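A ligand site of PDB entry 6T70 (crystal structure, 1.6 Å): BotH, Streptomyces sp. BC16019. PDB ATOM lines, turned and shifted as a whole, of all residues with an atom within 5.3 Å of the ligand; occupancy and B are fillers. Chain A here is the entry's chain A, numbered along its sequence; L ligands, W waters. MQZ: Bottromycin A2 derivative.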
ATOM      1  N   VAL A  58      -2.798  16.368 -20.352  1.00  0.00           N
ATOM      2  CA  VAL A  58      -3.484  17.245 -19.380  1.00  0.00           C
ATOM      3  C   VAL A  58      -4.914  17.498 -19.804  1.00  0.00           C
ATOM      4  O   VAL A  58      -5.850  17.460 -18.969  1.00  0.00           O
ATOM      5  CB  VAL A  58      -2.712  18.576 -19.224  1.00  0.00           C
ATOM      6  CG1 VAL A  58      -3.533  19.569 -18.398  1.00  0.00           C
ATOM      7  CG2 VAL A  58      -1.367  18.350 -18.575  1.00  0.00           C
ATOM      8  N   ALA A  59      -5.112  17.862 -21.058  1.00  0.00           N
ATOM      9  CA  ALA A  59      -6.422  18.265 -21.587  1.00  0.00           C
ATOM     10  C   ALA A  59      -7.073  17.105 -22.345  1.00  0.00           C
ATOM     11  O   ALA A  59      -7.718  17.342 -23.347  1.00  0.00           O
ATOM     12  CB  ALA A  59      -6.259  19.484 -22.493  1.00  0.00           C
ATOM     13  N   PHE A 126       2.353  13.241 -24.202  1.00  0.00           N
ATOM     14  CA  PHE A 126       2.611  14.627 -23.786  1.00  0.00           C
ATOM     15  C   PHE A 126       2.894  14.583 -22.288  1.00  0.00           C
ATOM     16  O   PHE A 126       3.805  13.825 -21.874  1.00  0.00           O
ATOM     17  CB  PHE A 126       1.503  15.558 -24.254  1.00  0.00           C
ATOM     18  CG  PHE A 126       1.419  15.656 -25.756  1.00  0.00           C
ATOM     19  CD1 PHE A 126       2.318  16.429 -26.471  1.00  0.00           C
ATOM     20  CD2 PHE A 126       0.466  14.941 -26.457  1.00  0.00           C
ATOM     21  CE1 PHE A 126       2.260  16.524 -27.851  1.00  0.00           C
ATOM     22  CE2 PHE A 126       0.401  15.020 -27.842  1.00  0.00           C
ATOM     23  CZ  PHE A 126       1.310  15.787 -28.550  1.00  0.00           C
ATOM     24  N   PHE A 127       2.199  15.353 -21.424  1.00  0.00           N
ATOM     25  CA  PHE A 127       2.582  15.275 -20.019  1.00  0.00           C
ATOM     26  C   PHE A 127       2.367  13.871 -19.482  1.00  0.00           C
ATOM     27  O   PHE A 127       3.020  13.483 -18.528  1.00  0.00           O
ATOM     28  CB  PHE A 127       1.830  16.283 -19.191  1.00  0.00           C
ATOM     29  CG  PHE A 127       2.432  16.475 -17.826  1.00  0.00           C
ATOM     30  CD1 PHE A 127       3.689  16.997 -17.689  1.00  0.00           C
ATOM     31  CD2 PHE A 127       1.758  16.062 -16.685  1.00  0.00           C
ATOM     32  CE1 PHE A 127       4.277  17.138 -16.455  1.00  0.00           C
ATOM     33  CE2 PHE A 127       2.336  16.201 -15.454  1.00  0.00           C
ATOM     34  CZ  PHE A 127       3.574  16.737 -15.332  1.00  0.00           C
ATOM     35  N   ARG A 130       5.672  12.272 -19.412  1.00  0.00           N
ATOM     36  CA  ARG A 130       6.449  12.644 -18.239  1.00  0.00           C
ATOM     37  C   ARG A 130       5.999  11.841 -17.031  1.00  0.00           C
ATOM     38  O   ARG A 130       6.812  11.361 -16.261  1.00  0.00           O
ATOM     39  CB  ARG A 130       6.298  14.130 -17.939  1.00  0.00           C
ATOM     40  CG  ARG A 130       6.755  15.080 -19.016  1.00  0.00           C
ATOM     41  CD  ARG A 130       8.270  15.290 -18.987  1.00  0.00           C
ATOM     42  NE  ARG A 130       8.781  16.020 -17.801  1.00  0.00           N
ATOM     43  CZ  ARG A 130      10.017  16.495 -17.715  1.00  0.00           C
ATOM     44  NH1 ARG A 130      10.838  16.358 -18.735  1.00  0.00           N
ATOM     45  NH2 ARG A 130      10.437  17.148 -16.622  1.00  0.00           N
ATOM     46  N   CYS A 149       6.186  12.368 -27.244  1.00  0.00           N
ATOM     47  CA  CYS A 149       6.295  13.812 -27.386  1.00  0.00           C
ATOM     48  C   CYS A 149       6.554  14.512 -26.067  1.00  0.00           C
ATOM     49  O   CYS A 149       6.159  15.648 -25.883  1.00  0.00           O
ATOM     50  CB  CYS A 149       5.056  14.399 -28.059  1.00  0.00           C
ATOM     51  SG  CYS A 149       4.977  13.886 -29.833  1.00  0.00           S
ATOM     52  N   ALA A 150       7.261  13.845 -25.175  1.00  0.00           N
ATOM     53  CA  ALA A 150       7.807  14.493 -23.987  1.00  0.00           C
ATOM     54  C   ALA A 150       9.140  13.819 -23.670  1.00  0.00           C
ATOM     55  O   ALA A 150       9.290  12.607 -23.864  1.00  0.00           O
ATOM     56  CB  ALA A 150       6.876  14.387 -22.784  1.00  0.00           C
ATOM     57  N   VAL A 155      13.418  21.035 -16.863  1.00  0.00           N
ATOM     58  CA  VAL A 155      12.970  22.187 -17.635  1.00  0.00           C
ATOM     59  C   VAL A 155      12.849  23.375 -16.698  1.00  0.00           C
ATOM     60  O   VAL A 155      12.688  23.213 -15.497  1.00  0.00           O
ATOM     61  CB  VAL A 155      11.650  21.933 -18.325  1.00  0.00           C
ATOM     62  CG1 VAL A 155      11.784  20.848 -19.360  1.00  0.00           C
ATOM     63  CG2 VAL A 155      10.576  21.528 -17.312  1.00  0.00           C
ATOM     64  N   GLU A 156      12.973  24.565 -17.264  1.00  0.00           N
ATOM     65  CA  GLU A 156      12.686  25.813 -16.571  1.00  0.00           C
ATOM     66  C   GLU A 156      11.253  26.204 -16.911  1.00  0.00           C
ATOM     67  O   GLU A 156      10.928  26.427 -18.080  1.00  0.00           O
ATOM     68  CB  GLU A 156      13.642  26.932 -16.983  1.00  0.00           C
ATOM     69  CG  GLU A 156      13.410  28.247 -16.265  1.00  0.00           C
ATOM     70  CD  GLU A 156      13.859  29.448 -17.087  1.00  0.00           C
ATOM     71  OE1 GLU A 156      13.046  30.388 -17.250  1.00  0.00           O
ATOM     72  OE2 GLU A 156      15.006  29.454 -17.582  1.00  0.00           O
ATOM     73  N   ILE A 157      10.384  26.239 -15.915  1.00  0.00           N
ATOM     74  CA  ILE A 157       8.978  26.552 -16.122  1.00  0.00           C
ATOM     75  C   ILE A 157       8.750  28.011 -15.731  1.00  0.00           C
ATOM     76  O   ILE A 157       9.003  28.363 -14.574  1.00  0.00           O
ATOM     77  CB  ILE A 157       8.081  25.607 -15.320  1.00  0.00           C
ATOM     78  CG1 ILE A 157       8.374  24.168 -15.739  1.00  0.00           C
ATOM     79  CG2 ILE A 157       6.618  25.960 -15.534  1.00  0.00           C
ATOM     80  CD1 ILE A 157       7.416  23.126 -15.191  1.00  0.00           C
ATOM     81  N   PRO A 158       8.311  28.881 -16.639  1.00  0.00           N
ATOM     82  CA  PRO A 158       8.054  30.275 -16.253  1.00  0.00           C
ATOM     83  C   PRO A 158       6.751  30.363 -15.462  1.00  0.00           C
ATOM     84  O   PRO A 158       5.687  30.038 -15.983  1.00  0.00           O
ATOM     85  CB  PRO A 158       7.955  31.003 -17.597  1.00  0.00           C
ATOM     86  CG  PRO A 158       8.246  30.011 -18.665  1.00  0.00           C
ATOM     87  CD  PRO A 158       8.047  28.639 -18.081  1.00  0.00           C
ATOM     88  N   ALA A 161       4.039  32.770 -17.103  1.00  0.00           N
ATOM     89  CA  ALA A 161       3.350  32.273 -18.290  1.00  0.00           C
ATOM     90  C   ALA A 161       2.399  31.146 -17.944  1.00  0.00           C
ATOM     91  O   ALA A 161       1.280  31.076 -18.475  1.00  0.00           O
ATOM     92  CB  ALA A 161       4.379  31.810 -19.326  1.00  0.00           C
ATOM     93  N   VAL A 162       2.821  30.232 -17.064  1.00  0.00           N
ATOM     94  CA  VAL A 162       1.929  29.141 -16.685  1.00  0.00           C
ATOM     95  C   VAL A 162       0.701  29.650 -15.968  1.00  0.00           C
ATOM     96  O   VAL A 162      -0.416  29.155 -16.199  1.00  0.00           O
ATOM     97  CB  VAL A 162       2.697  28.093 -15.848  1.00  0.00           C
ATOM     98  CG1 VAL A 162       1.729  27.089 -15.242  1.00  0.00           C
ATOM     99  CG2 VAL A 162       3.750  27.394 -16.699  1.00  0.00           C
ATOM    100  N   GLU A 165      -1.599  30.970 -18.538  1.00  0.00           N
ATOM    101  CA  GLU A 165      -2.298  29.901 -19.246  1.00  0.00           C
ATOM    102  C   GLU A 165      -3.388  29.298 -18.371  1.00  0.00           C
ATOM    103  O   GLU A 165      -4.476  28.955 -18.863  1.00  0.00           O
ATOM    104  CB  GLU A 165      -1.319  28.834 -19.687  1.00  0.00           C
ATOM    105  CG  GLU A 165      -1.939  27.764 -20.566  1.00  0.00           C
ATOM    106  CD  GLU A 165      -1.017  27.393 -21.710  1.00  0.00           C
ATOM    107  OE1 GLU A 165      -1.212  27.956 -22.808  1.00  0.00           O
ATOM    108  OE2 GLU A 165      -0.110  26.561 -21.498  1.00  0.00           O
ATOM    109  N   VAL A 169      -7.419  28.990 -19.508  1.00  0.00           N
ATOM    110  CA  VAL A 169      -8.101  27.725 -19.751  1.00  0.00           C
ATOM    111  C   VAL A 169      -9.217  27.454 -18.752  1.00  0.00           C
ATOM    112  O   VAL A 169     -10.095  26.624 -19.032  1.00  0.00           O
ATOM    113  CB  VAL A 169      -7.147  26.528 -19.733  1.00  0.00           C
ATOM    114  CG1 VAL A 169      -6.119  26.611 -20.886  1.00  0.00           C
ATOM    115  CG2 VAL A 169      -6.429  26.381 -18.380  1.00  0.00           C
ATOM    116  N   TYR A 177     -10.444  28.570 -26.186  1.00  0.00           N
ATOM    117  CA  TYR A 177      -9.034  28.927 -26.274  1.00  0.00           C
ATOM    118  C   TYR A 177      -8.195  27.725 -26.674  1.00  0.00           C
ATOM    119  O   TYR A 177      -7.399  27.804 -27.620  1.00  0.00           O
ATOM    120  CB  TYR A 177      -8.592  29.490 -24.917  1.00  0.00           C
ATOM    121  CG  TYR A 177      -7.102  29.667 -24.701  1.00  0.00           C
ATOM    122  CD1 TYR A 177      -6.432  30.801 -25.146  1.00  0.00           C
ATOM    123  CD2 TYR A 177      -6.380  28.710 -24.013  1.00  0.00           C
ATOM    124  CE1 TYR A 177      -5.072  30.957 -24.936  1.00  0.00           C
ATOM    125  CE2 TYR A 177      -5.019  28.849 -23.792  1.00  0.00           C
ATOM    126  CZ  TYR A 177      -4.366  29.975 -24.249  1.00  0.00           C
ATOM    127  OH  TYR A 177      -3.017  30.109 -24.016  1.00  0.00           O
ATOM    128  N   LEU A 178      -8.374  26.591 -26.003  1.00  0.00           N
ATOM    129  CA  LEU A 178      -7.619  25.397 -26.313  1.00  0.00           C
ATOM    130  C   LEU A 178      -7.985  24.830 -27.679  1.00  0.00           C
ATOM    131  O   LEU A 178      -7.097  24.434 -28.460  1.00  0.00           O
ATOM    132  CB  LEU A 178      -7.839  24.347 -25.239  1.00  0.00           C
ATOM    133  CG  LEU A 178      -7.170  24.605 -23.905  1.00  0.00           C
ATOM    134  CD1 LEU A 178      -7.530  23.509 -22.910  1.00  0.00           C
ATOM    135  CD2 LEU A 178      -5.658  24.658 -24.060  1.00  0.00           C
ATOM    136  N   HIS A 181      -6.437  27.058 -30.390  1.00  0.00           N
ATOM    137  CA  HIS A 181      -4.988  26.914 -30.476  1.00  0.00           C
ATOM    138  C   HIS A 181      -4.580  25.551 -31.004  1.00  0.00           C
ATOM    139  O   HIS A 181      -3.707  25.456 -31.873  1.00  0.00           O
ATOM    140  CB  HIS A 181      -4.380  27.181 -29.106  1.00  0.00           C
ATOM    141  CG  HIS A 181      -4.215  28.643 -28.807  1.00  0.00           C
ATOM    142  ND1 HIS A 181      -3.015  29.310 -28.956  1.00  0.00           N
ATOM    143  CD2 HIS A 181      -5.104  29.568 -28.368  1.00  0.00           C
ATOM    144  CE1 HIS A 181      -3.163  30.569 -28.619  1.00  0.00           C
ATOM    145  NE2 HIS A 181      -4.423  30.761 -28.253  1.00  0.00           N
ATOM    146  N   PHE A 182      -5.216  24.476 -30.525  1.00  0.00           N
ATOM    147  CA  PHE A 182      -4.840  23.156 -31.042  1.00  0.00           C
ATOM    148  C   PHE A 182      -5.251  23.003 -32.505  1.00  0.00           C
ATOM    149  O   PHE A 182      -4.512  22.430 -33.309  1.00  0.00           O
ATOM    150  CB  PHE A 182      -5.439  22.054 -30.187  1.00  0.00           C
ATOM    151  CG  PHE A 182      -4.769  21.856 -28.855  1.00  0.00           C
ATOM    152  CD1 PHE A 182      -3.395  21.929 -28.735  1.00  0.00           C
ATOM    153  CD2 PHE A 182      -5.508  21.603 -27.741  1.00  0.00           C
ATOM    154  CE1 PHE A 182      -2.790  21.748 -27.498  1.00  0.00           C
ATOM    155  CE2 PHE A 182      -4.923  21.436 -26.520  1.00  0.00           C
ATOM    156  CZ  PHE A 182      -3.559  21.515 -26.407  1.00  0.00           C
ATOM    157  N   ARG A 185      -2.745  24.722 -34.699  1.00  0.00           N
ATOM    158  CA  ARG A 185      -1.443  24.019 -34.734  1.00  0.00           C
ATOM    159  C   ARG A 185      -1.558  22.606 -35.308  1.00  0.00           C
ATOM    160  O   ARG A 185      -0.579  21.831 -35.232  1.00  0.00           O
ATOM    161  CB  ARG A 185      -0.827  24.039 -33.339  1.00  0.00           C
ATOM    162  CG  ARG A 185      -0.438  25.456 -32.885  1.00  0.00           C
ATOM    163  CD  ARG A 185       0.023  25.528 -31.439  1.00  0.00           C
ATOM    164  NE  ARG A 185       0.967  26.634 -31.216  1.00  0.00           N
ATOM    165  CZ  ARG A 185       0.773  27.672 -30.393  1.00  0.00           C
ATOM    166  NH1 ARG A 185      -0.340  27.770 -29.669  1.00  0.00           N
ATOM    167  NH2 ARG A 185       1.712  28.599 -30.279  1.00  0.00           N
ATOM    168  N   MET A 191      -7.892  15.195 -30.433  1.00  0.00           N
ATOM    169  CA  MET A 191      -7.162  16.007 -29.461  1.00  0.00           C
ATOM    170  C   MET A 191      -7.823  17.349 -29.277  1.00  0.00           C
ATOM    171  O   MET A 191      -7.944  17.834 -28.134  1.00  0.00           O
ATOM    172  CB  MET A 191      -5.719  16.169 -29.920  1.00  0.00           C
ATOM    173  CG  MET A 191      -4.838  16.924 -28.972  1.00  0.00           C
ATOM    174  SD  MET A 191      -3.135  16.629 -29.518  1.00  0.00           S
ATOM    175  CE  MET A 191      -2.435  18.146 -28.950  1.00  0.00           C
ATOM    176  N   THR A 207      -2.949  22.947 -14.777  1.00  0.00           N
ATOM    177  CA  THR A 207      -1.894  23.830 -15.300  1.00  0.00           C
ATOM    178  C   THR A 207      -1.051  24.374 -14.142  1.00  0.00           C
ATOM    179  O   THR A 207       0.175  24.312 -14.183  1.00  0.00           O
ATOM    180  CB  THR A 207      -2.554  24.966 -16.084  1.00  0.00           C
ATOM    181  OG1 THR A 207      -3.274  24.382 -17.199  1.00  0.00           O
ATOM    182  CG2 THR A 207      -1.539  25.931 -16.587  1.00  0.00           C
ATOM    183  N   LEU A 210       1.576  22.036 -12.500  1.00  0.00           N
ATOM    184  CA  LEU A 210       2.892  21.880 -13.106  1.00  0.00           C
ATOM    185  C   LEU A 210       3.975  22.605 -12.342  1.00  0.00           C
ATOM    186  O   LEU A 210       5.166  22.315 -12.507  1.00  0.00           O
ATOM    187  CB  LEU A 210       2.867  22.378 -14.549  1.00  0.00           C
ATOM    188  CG  LEU A 210       1.930  21.629 -15.483  1.00  0.00           C
ATOM    189  CD1 LEU A 210       1.818  22.377 -16.833  1.00  0.00           C
ATOM    190  CD2 LEU A 210       2.383  20.176 -15.716  1.00  0.00           C
ATOM    191  N   SER A 214       6.896  19.221 -11.595  1.00  0.00           N
ATOM    192  CA  SER A 214       7.022  18.723 -12.939  1.00  0.00           C
ATOM    193  C   SER A 214       8.304  19.186 -13.622  1.00  0.00           C
ATOM    194  O   SER A 214       8.604  18.706 -14.732  1.00  0.00           O
ATOM    195  CB  SER A 214       5.836  19.180 -13.795  1.00  0.00           C
ATOM    196  OG  SER A 214       6.103  20.406 -14.423  1.00  0.00           O
ATOM    197  N   ARG A 260       5.696  18.766 -32.544  1.00  0.00           N
ATOM    198  CA  ARG A 260       5.200  17.780 -31.592  1.00  0.00           C
ATOM    199  C   ARG A 260       3.707  17.587 -31.687  1.00  0.00           C
ATOM    200  O   ARG A 260       3.208  16.455 -31.595  1.00  0.00           O
ATOM    201  CB  ARG A 260       5.546  18.194 -30.147  1.00  0.00           C
ATOM    202  CG  ARG A 260       6.901  17.776 -29.716  1.00  0.00           C
ATOM    203  CD  ARG A 260       7.238  18.285 -28.310  1.00  0.00           C
ATOM    204  NE  ARG A 260       8.640  18.568 -28.254  1.00  0.00           N
ATOM    205  CZ  ARG A 260       9.260  19.183 -27.230  1.00  0.00           C
ATOM    206  NH1 ARG A 260       8.584  19.524 -26.144  1.00  0.00           N
ATOM    207  NH2 ARG A 260      10.534  19.419 -27.311  1.00  0.00           N
ATOM    208  N   ILE A 261       2.960  18.680 -31.804  1.00  0.00           N
ATOM    209  CA  ILE A 261       1.517  18.581 -31.831  1.00  0.00           C
ATOM    210  C   ILE A 261       1.074  17.807 -33.053  1.00  0.00           C
ATOM    211  O   ILE A 261       0.184  16.967 -32.984  1.00  0.00           O
ATOM    212  CB  ILE A 261       0.868  19.975 -31.788  1.00  0.00           C
ATOM    213  CG1 ILE A 261       0.861  20.503 -30.349  1.00  0.00           C
ATOM    214  CG2 ILE A 261      -0.560  19.914 -32.341  1.00  0.00           C
ATOM    215  CD1 ILE A 261       0.463  21.952 -30.219  1.00  0.00           C
HETATM  216  C10 MQZ L   1      -0.096  25.346 -24.816  1.00  0.00           C
HETATM  217  C13 MQZ L   1      -2.899  27.086 -26.392  1.00  0.00           C
HETATM  218  C15 MQZ L   1       2.223  24.919 -23.746  1.00  0.00           C
HETATM  219  C17 MQZ L   1       3.662  26.527 -22.355  1.00  0.00           C
HETATM  220  C20 MQZ L   1       2.484  28.476 -21.364  1.00  0.00           C
HETATM  221  C21 MQZ L   1       3.850  28.719 -23.386  1.00  0.00           C
HETATM  222  C22 MQZ L   1       3.699  25.400 -21.157  1.00  0.00           C
HETATM  223  C24 MQZ L   1       2.172  24.419 -19.393  1.00  0.00           C
HETATM  224  C28 MQZ L   1       5.994  24.440 -21.569  1.00  0.00           C
HETATM  225  C01 MQZ L   1      -2.920  22.031 -22.206  1.00  0.00           C
HETATM  226  C02 MQZ L   1      -2.075  22.348 -21.012  1.00  0.00           C
HETATM  227  C03 MQZ L   1      -2.182  23.771 -20.482  1.00  0.00           C
HETATM  228  C04 MQZ L   1      -0.866  24.011 -19.760  1.00  0.00           C
HETATM  229  C06 MQZ L   1      -0.572  22.159 -21.261  1.00  0.00           C
HETATM  230  C07 MQZ L   1      -0.119  22.517 -22.725  1.00  0.00           C
HETATM  231  C09 MQZ L   1       0.873  24.414 -24.234  1.00  0.00           C
HETATM  232  C11 MQZ L   1      -1.376  24.667 -25.243  1.00  0.00           C
HETATM  233  C18 MQZ L   1       3.720  27.941 -22.049  1.00  0.00           C
HETATM  234  C19 MQZ L   1       4.970  28.165 -21.202  1.00  0.00           C
HETATM  235  C25 MQZ L   1       1.497  23.254 -20.230  1.00  0.00           C
HETATM  236  C29 MQZ L   1       7.116  24.433 -20.517  1.00  0.00           C
HETATM  237  C30 MQZ L   1       7.045  25.650 -19.595  1.00  0.00           C
HETATM  238  C31 MQZ L   1       6.948  23.199 -19.616  1.00  0.00           C
HETATM  239  C32 MQZ L   1       8.516  24.360 -21.148  1.00  0.00           C
HETATM  240  C33 MQZ L   1       6.072  23.105 -22.326  1.00  0.00           C
HETATM  241  C35 MQZ L   1       5.193  20.678 -22.503  1.00  0.00           C
HETATM  242  C36 MQZ L   1       4.615  20.469 -23.912  1.00  0.00           C
HETATM  243  C38 MQZ L   1       3.193  20.977 -25.822  1.00  0.00           C
HETATM  244  C39 MQZ L   1       1.810  20.405 -25.771  1.00  0.00           C
HETATM  245  C41 MQZ L   1       0.160  19.010 -25.191  1.00  0.00           C
HETATM  246  C42 MQZ L   1      -0.521  19.797 -26.066  1.00  0.00           C
HETATM  247  C44 MQZ L   1       3.363  22.210 -26.634  1.00  0.00           C
HETATM  248  C45 MQZ L   1       4.818  22.238 -27.077  1.00  0.00           C
HETATM  249  C47 MQZ L   1       6.251  22.249 -28.927  1.00  0.00           C
HETATM  250  C50 MQZ L   1       4.487  19.717 -21.465  1.00  0.00           C
HETATM  251  C51 MQZ L   1       5.285  19.693 -20.202  1.00  0.00           C
HETATM  252  C52 MQZ L   1       6.567  19.102 -20.193  1.00  0.00           C
HETATM  253  C53 MQZ L   1       7.355  19.064 -19.060  1.00  0.00           C
HETATM  254  C54 MQZ L   1       6.900  19.630 -17.884  1.00  0.00           C
HETATM  255  C55 MQZ L   1       5.642  20.228 -17.866  1.00  0.00           C
HETATM  256  C56 MQZ L   1       4.866  20.271 -19.010  1.00  0.00           C
HETATM  257  C57 MQZ L   1       4.353  18.298 -21.992  1.00  0.00           C
HETATM  258  N05 MQZ L   1       0.116  23.126 -20.416  1.00  0.00           N
HETATM  259  N08 MQZ L   1       0.374  23.817 -22.928  1.00  0.00           N
HETATM  260  N16 MQZ L   1       2.375  26.051 -22.965  1.00  0.00           N
HETATM  261  N23 MQZ L   1       2.509  25.372 -20.402  1.00  0.00           N
HETATM  262  N27 MQZ L   1       4.669  24.569 -20.949  1.00  0.00           N
HETATM  263  N34 MQZ L   1       5.200  22.051 -21.928  1.00  0.00           N
HETATM  264  N37 MQZ L   1       3.670  21.282 -24.459  1.00  0.00           N
HETATM  265  N40 MQZ L   1       1.505  19.362 -25.027  1.00  0.00           N
HETATM  266  O14 MQZ L   1      -1.851  25.173 -27.958  1.00  0.00           O
HETATM  267  O26 MQZ L   1       2.179  22.478 -20.884  1.00  0.00           O
HETATM  268  O46 MQZ L   1       5.030  21.805 -28.347  1.00  0.00           O
HETATM  269  O48 MQZ L   1       5.768  22.569 -26.376  1.00  0.00           O
HETATM  270  O49 MQZ L   1       5.035  19.558 -24.593  1.00  0.00           O
HETATM  271  O58 MQZ L   1       6.859  22.926 -23.207  1.00  0.00           O
HETATM  272  O59 MQZ L   1       3.190  24.249 -24.038  1.00  0.00           O
HETATM  273  O60 MQZ L   1      -0.205  21.690 -23.631  1.00  0.00           O
HETATM  274  S12 MQZ L   1      -2.070  25.628 -26.581  1.00  0.00           S
HETATM  275  S43 MQZ L   1       0.499  21.019 -26.709  1.00  0.00           S
HETATM  276  O   HOH W   1       8.735  20.841 -23.664  1.00  0.00           O
HETATM  277  O   HOH W   2       6.800  17.927 -24.589  1.00  0.00           O
HETATM  278  O   HOH W   3       4.104  21.425 -31.161  1.00  0.00           O
HETATM  279  O   HOH W   4       9.406  21.524 -29.905  1.00  0.00           O
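O of Leu 210 is in hydrogen-bond range of OG of Ser 214, at 2.9 Å.
The side-chain sulfur of Cys 149 lies within hydrogen-bond range of the backbone carbonyl oxygen of Arg 260 (3.6 Å).
The backbone carbonyl oxygen (O) of Ser 214 is in hydrogen-bond range of the guanidinium group (NH2) of Arg 130.
The side-chain carboxylate (OE1) of Glu 165 lies within hydrogen-bond range of the side-chain hydroxyl (OH) of Tyr 177 (3.1 Å).
A ring nitrogen (ND1) of His 181 is in hydrogen-bond range of the guanidinium group (NH1) of Arg 185 (3.2 Å).
NH1 of Arg 185 is in hydrogen-bond range of O14 of the ligand (3.5 Å).
A nitrogen (N16) of the ligand is in hydrogen-bond range of the side-chain carboxylate (OE2) of Glu 165 (2.9 Å).
Water W2 lies within hydrogen-bond range of an oxygen (O49) of the ligand (2.4 Å), the backbone carbonyl oxygen of Cys 149 (2.7 Å) and the guanidinium group of Arg 260 (2.9 Å).
Water W1 lies within hydrogen-bond range of the guanidinium group (NH1) of Arg 260 and an oxygen (O58) of the ligand.
Water W3 lies within hydrogen-bond range of O46 of the ligand (3.0 Å), N of Ile 261 (3.0 Å) and N of Arg 260 (3.4 Å).
Phe 126 touches the ligand (CD1 to N40, 3.4 Å).
Phe 127 touches the ligand (CE1 to C55, 3.7 Å).
Arg 130 touches the ligand.
Pro 158 touches the ligand.
CE2 of Tyr 177 touches C13 of the ligand, at 3.8 Å.
His 181 touches the ligand.
Phe 182 touches the ligand (CE1 to C42, 3.3 Å).
CE of Met 191 touches C42 of the ligand, at 3.8 Å.
Thr 207 touches the ligand (OG1 to C03, 3.5 Å).
Leu 210 touches the ligand (CD1 to C24, 3.3 Å).
OG of Ser 214 touches C55 of the ligand (3.5 Å).
Arg 260 touches the ligand.
CD1 of Ile 261 touches S43 of the ligand, at 3.6 Å.
Within 4 Å of the ligand: Phe 126, Phe 127, Arg 130, Pro 158, Glu 165, Tyr 177, His 181, Phe 182, Arg 185, Met 191, Thr 207, Leu 210, Ser 214, Arg 260 and Ile 261.
The nearest printed residue that does not touch the ligand is Ala 161 (4.1 Å).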
